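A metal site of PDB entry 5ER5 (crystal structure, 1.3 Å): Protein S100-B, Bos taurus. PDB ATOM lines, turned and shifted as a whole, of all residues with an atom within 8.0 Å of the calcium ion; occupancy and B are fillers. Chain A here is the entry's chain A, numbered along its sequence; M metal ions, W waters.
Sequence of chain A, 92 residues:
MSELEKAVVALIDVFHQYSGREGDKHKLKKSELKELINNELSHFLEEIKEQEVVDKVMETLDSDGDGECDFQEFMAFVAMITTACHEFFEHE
Within 4 Å of the calcium ion: Asp 62, Asp 64, Asp 66, Glu 68 and Glu 73.
The nearest printed residue that does not touch the calcium ion is Asp 70 (4.4 Å).
The backbone NH (N) of Gly 65 lies close to the side-chain carboxylate (OD1) of Asp 62 (3.2 Å).
The side-chain carboxylate (OD2) of Asp 62 lies within hydrogen-bond range of the backbone NH (N) of Gly 67 (2.7 Å).
The side-chain carboxylate (OD2) of Asp 66 lies within salt-bridge range of the side-chain amino group (NZ) of Lys 27.
N of Glu 73 lies within hydrogen-bond range of OD1 of Asp 70, 2.9 Å away.
The backbone NH of Ser 63 lies close to the side-chain carboxylate of Glu 73 (3.2 Å).
OD1 of Asp 62 is bound to the calcium ion, at 2.3 Å.
O of Glu 68 binds the calcium ion, at 2.3 Å.
OD1 of Asp 64 binds the calcium ion (2.3 Å).
OD1 of Asp 66 is bound to the calcium ion, 2.4 Å away.
The side-chain carboxylate (OE1) of Glu 73 binds the calcium ion (2.4 Å).
Water W1 is bound to the calcium ion (2.4 Å).
OE2 of Glu 73 binds the calcium ion, at 2.6 Å.
The calcium ion has seven donor atoms within binding distance.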
ATOM      1  N   LYS A  27     -32.493 -13.027 -14.274  1.00  0.00           N
ATOM      2  CA  LYS A  27     -31.238 -13.583 -14.756  1.00  0.00           C
ATOM      3  C   LYS A  27     -30.107 -12.600 -14.503  1.00  0.00           C
ATOM      4  O   LYS A  27     -30.318 -11.388 -14.380  1.00  0.00           O
ATOM      5  CB  LYS A  27     -31.296 -13.886 -16.264  1.00  0.00           C
ATOM      6  CG  LYS A  27     -32.408 -14.826 -16.681  1.00  0.00           C
ATOM      7  CD  LYS A  27     -32.350 -15.113 -18.173  1.00  0.00           C
ATOM      8  CE  LYS A  27     -33.572 -15.859 -18.697  1.00  0.00           C
ATOM      9  NZ  LYS A  27     -33.678 -15.705 -20.177  1.00  0.00           N
ATOM     10  N   LEU A  28     -28.886 -13.153 -14.440  1.00  0.00           N
ATOM     11  CA  LEU A  28     -27.661 -12.370 -14.287  1.00  0.00           C
ATOM     12  C   LEU A  28     -27.063 -12.093 -15.668  1.00  0.00           C
ATOM     13  O   LEU A  28     -26.698 -13.032 -16.391  1.00  0.00           O
ATOM     14  CB  LEU A  28     -26.632 -13.166 -13.492  1.00  0.00           C
ATOM     15  CG  LEU A  28     -26.985 -13.570 -12.075  1.00  0.00           C
ATOM     16  CD1 LEU A  28     -26.058 -14.684 -11.618  1.00  0.00           C
ATOM     17  CD2 LEU A  28     -26.911 -12.402 -11.150  1.00  0.00           C
ATOM     18  N   MET A  58     -18.980 -16.235 -18.049  1.00  0.00           N
ATOM     19  CA  MET A  58     -20.355 -16.347 -18.536  1.00  0.00           C
ATOM     20  C   MET A  58     -20.466 -17.425 -19.597  1.00  0.00           C
ATOM     21  O   MET A  58     -21.416 -18.210 -19.590  1.00  0.00           O
ATOM     22  CB  MET A  58     -20.829 -15.014 -19.110  1.00  0.00           C
ATOM     23  CG  MET A  58     -22.272 -15.070 -19.667  1.00  0.00           C
ATOM     24  SD  MET A  58     -23.543 -15.328 -18.411  1.00  0.00           S
ATOM     25  CE  MET A  58     -23.731 -13.653 -17.771  1.00  0.00           C
ATOM     26  N   LEU A  61     -20.643 -20.881 -17.931  1.00  0.00           N
ATOM     27  CA  LEU A  61     -21.810 -21.278 -17.160  1.00  0.00           C
ATOM     28  C   LEU A  61     -23.137 -21.128 -17.894  1.00  0.00           C
ATOM     29  O   LEU A  61     -24.156 -21.631 -17.404  1.00  0.00           O
ATOM     30  CB  LEU A  61     -21.853 -20.567 -15.804  1.00  0.00           C
ATOM     31  CG  LEU A  61     -21.881 -19.049 -15.752  1.00  0.00           C
ATOM     32  CD1 LEU A  61     -23.182 -18.454 -16.308  1.00  0.00           C
ATOM     33  CD2 LEU A  61     -21.653 -18.634 -14.281  1.00  0.00           C
ATOM     34  N   ASP A  62     -23.143 -20.471 -19.053  1.00  0.00           N
ATOM     35  CA  ASP A  62     -24.374 -20.194 -19.802  1.00  0.00           C
ATOM     36  C   ASP A  62     -24.728 -21.420 -20.643  1.00  0.00           C
ATOM     37  O   ASP A  62     -24.551 -21.455 -21.862  1.00  0.00           O
ATOM     38  CB  ASP A  62     -24.216 -18.959 -20.659  1.00  0.00           C
ATOM     39  CG  ASP A  62     -25.449 -18.672 -21.495  1.00  0.00           C
ATOM     40  OD1 ASP A  62     -26.532 -19.116 -21.089  1.00  0.00           O
ATOM     41  OD2 ASP A  62     -25.324 -17.987 -22.528  1.00  0.00           O
ATOM     42  N   SER A  63     -25.298 -22.418 -19.961  1.00  0.00           N
ATOM     43  CA  SER A  63     -25.554 -23.719 -20.580  1.00  0.00           C
ATOM     44  C   SER A  63     -26.559 -23.621 -21.727  1.00  0.00           C
ATOM     45  O   SER A  63     -26.439 -24.353 -22.720  1.00  0.00           O
ATOM     46  CB  SER A  63     -26.042 -24.711 -19.528  1.00  0.00           C
ATOM     47  OG  SER A  63     -24.999 -25.001 -18.626  1.00  0.00           O
ATOM     48  N   ASP A  64     -27.556 -22.752 -21.611  1.00  0.00           N
ATOM     49  CA  ASP A  64     -28.587 -22.675 -22.642  1.00  0.00           C
ATOM     50  C   ASP A  64     -28.283 -21.651 -23.731  1.00  0.00           C
ATOM     51  O   ASP A  64     -29.040 -21.563 -24.702  1.00  0.00           O
ATOM     52  CB  ASP A  64     -29.981 -22.502 -22.030  1.00  0.00           C
ATOM     53  CG  ASP A  64     -30.202 -21.155 -21.371  1.00  0.00           C
ATOM     54  OD1 ASP A  64     -29.378 -20.234 -21.533  1.00  0.00           O
ATOM     55  OD2 ASP A  64     -31.251 -21.018 -20.692  1.00  0.00           O
ATOM     56  N   GLY A  65     -27.187 -20.901 -23.608  1.00  0.00           N
ATOM     57  CA  GLY A  65     -26.693 -20.074 -24.691  1.00  0.00           C
ATOM     58  C   GLY A  65     -27.378 -18.740 -24.853  1.00  0.00           C
ATOM     59  O   GLY A  65     -27.113 -18.061 -25.854  1.00  0.00           O
ATOM     60  N   ASP A  66     -28.226 -18.326 -23.914  1.00  0.00           N
ATOM     61  CA  ASP A  66     -28.986 -17.089 -24.079  1.00  0.00           C
ATOM     62  C   ASP A  66     -28.236 -15.849 -23.618  1.00  0.00           C
ATOM     63  O   ASP A  66     -28.793 -14.755 -23.657  1.00  0.00           O
ATOM     64  CB  ASP A  66     -30.368 -17.198 -23.403  1.00  0.00           C
ATOM     65  CG  ASP A  66     -30.295 -17.156 -21.878  1.00  0.00           C
ATOM     66  OD1 ASP A  66     -29.188 -17.211 -21.301  1.00  0.00           O
ATOM     67  OD2 ASP A  66     -31.373 -17.083 -21.244  1.00  0.00           O
ATOM     68  N   GLY A  67     -26.972 -15.990 -23.217  1.00  0.00           N
ATOM     69  CA  GLY A  67     -26.148 -14.858 -22.853  1.00  0.00           C
ATOM     70  C   GLY A  67     -26.298 -14.394 -21.423  1.00  0.00           C
ATOM     71  O   GLY A  67     -25.629 -13.442 -21.026  1.00  0.00           O
ATOM     72  N   GLU A  68     -27.162 -15.034 -20.638  1.00  0.00           N
ATOM     73  CA  GLU A  68     -27.304 -14.683 -19.233  1.00  0.00           C
ATOM     74  C   GLU A  68     -27.278 -15.949 -18.398  1.00  0.00           C
ATOM     75  O   GLU A  68     -27.389 -17.060 -18.916  1.00  0.00           O
ATOM     76  CB  GLU A  68     -28.591 -13.881 -18.991  1.00  0.00           C
ATOM     77  CG  GLU A  68     -28.656 -12.601 -19.824  1.00  0.00           C
ATOM     78  CD  GLU A  68     -29.417 -11.457 -19.177  1.00  0.00           C
ATOM     79  OE1 GLU A  68     -29.637 -11.466 -17.957  1.00  0.00           O
ATOM     80  OE2 GLU A  68     -29.760 -10.508 -19.915  1.00  0.00           O
ATOM     81  N   CYS A  69     -27.109 -15.767 -17.093  1.00  0.00           N
ATOM     82  CA  CYS A  69     -27.095 -16.880 -16.151  1.00  0.00           C
ATOM     83  C   CYS A  69     -28.418 -16.904 -15.396  1.00  0.00           C
ATOM     84  O   CYS A  69     -28.684 -16.010 -14.586  1.00  0.00           O
ATOM     85  CB  CYS A  69     -25.920 -16.721 -15.186  1.00  0.00           C
ATOM     86  SG  CYS A  69     -25.744 -18.078 -14.024  1.00  0.00           S
ATOM     87  N   ASP A  70     -29.247 -17.927 -15.639  1.00  0.00           N
ATOM     88  CA  ASP A  70     -30.502 -18.071 -14.904  1.00  0.00           C
ATOM     89  C   ASP A  70     -30.251 -18.802 -13.577  1.00  0.00           C
ATOM     90  O   ASP A  70     -29.117 -19.114 -13.218  1.00  0.00           O
ATOM     91  CB  ASP A  70     -31.591 -18.728 -15.756  1.00  0.00           C
ATOM     92  CG  ASP A  70     -31.285 -20.163 -16.139  1.00  0.00           C
ATOM     93  OD1 ASP A  70     -30.470 -20.831 -15.485  1.00  0.00           O
ATOM     94  OD2 ASP A  70     -31.908 -20.632 -17.113  1.00  0.00           O
ATOM     95  N   PHE A  71     -31.328 -19.060 -12.827  1.00  0.00           N
ATOM     96  CA  PHE A  71     -31.126 -19.598 -11.489  1.00  0.00           C
ATOM     97  C   PHE A  71     -30.539 -20.999 -11.523  1.00  0.00           C
ATOM     98  O   PHE A  71     -29.642 -21.321 -10.722  1.00  0.00           O
ATOM     99  CB  PHE A  71     -32.409 -19.582 -10.664  1.00  0.00           C
ATOM    100  CG  PHE A  71     -32.165 -19.973  -9.237  1.00  0.00           C
ATOM    101  CD1 PHE A  71     -31.474 -19.121  -8.396  1.00  0.00           C
ATOM    102  CD2 PHE A  71     -32.560 -21.207  -8.748  1.00  0.00           C
ATOM    103  CE1 PHE A  71     -31.208 -19.468  -7.088  1.00  0.00           C
ATOM    104  CE2 PHE A  71     -32.294 -21.559  -7.448  1.00  0.00           C
ATOM    105  CZ  PHE A  71     -31.617 -20.685  -6.621  1.00  0.00           C
ATOM    106  N   GLU A  73     -28.628 -22.275 -13.814  1.00  0.00           N
ATOM    107  CA  GLU A  73     -27.221 -22.149 -14.197  1.00  0.00           C
ATOM    108  C   GLU A  73     -26.383 -21.610 -13.037  1.00  0.00           C
ATOM    109  O   GLU A  73     -25.220 -21.986 -12.872  1.00  0.00           O
ATOM    110  CB  GLU A  73     -27.092 -21.258 -15.433  1.00  0.00           C
ATOM    111  CG  GLU A  73     -27.698 -21.893 -16.679  1.00  0.00           C
ATOM    112  CD  GLU A  73     -27.949 -20.907 -17.820  1.00  0.00           C
ATOM    113  OE1 GLU A  73     -28.003 -19.693 -17.577  1.00  0.00           O
ATOM    114  OE2 GLU A  73     -28.106 -21.358 -18.976  1.00  0.00           O
ATOM    115  N   PHE A  74     -26.957 -20.702 -12.244  1.00  0.00           N
ATOM    116  CA  PHE A  74     -26.267 -20.199 -11.068  1.00  0.00           C
ATOM    117  C   PHE A  74     -26.025 -21.317 -10.058  1.00  0.00           C
ATOM    118  O   PHE A  74     -24.932 -21.438  -9.500  1.00  0.00           O
ATOM    119  CB  PHE A  74     -27.062 -19.069 -10.425  1.00  0.00           C
ATOM    120  CG  PHE A  74     -26.490 -18.581  -9.139  1.00  0.00           C
ATOM    121  CD1 PHE A  74     -25.296 -17.890  -9.119  1.00  0.00           C
ATOM    122  CD2 PHE A  74     -27.132 -18.823  -7.931  1.00  0.00           C
ATOM    123  CE1 PHE A  74     -24.743 -17.456  -7.917  1.00  0.00           C
ATOM    124  CE2 PHE A  74     -26.595 -18.377  -6.738  1.00  0.00           C
ATOM    125  CZ  PHE A  74     -25.397 -17.687  -6.740  1.00  0.00           C
HETATM  126 CA    CA M   1     -28.449 -18.929 -19.814  1.00  0.00          CA
HETATM  127  O   HOH W   1     -30.690 -18.591 -18.976  1.00  0.00           O
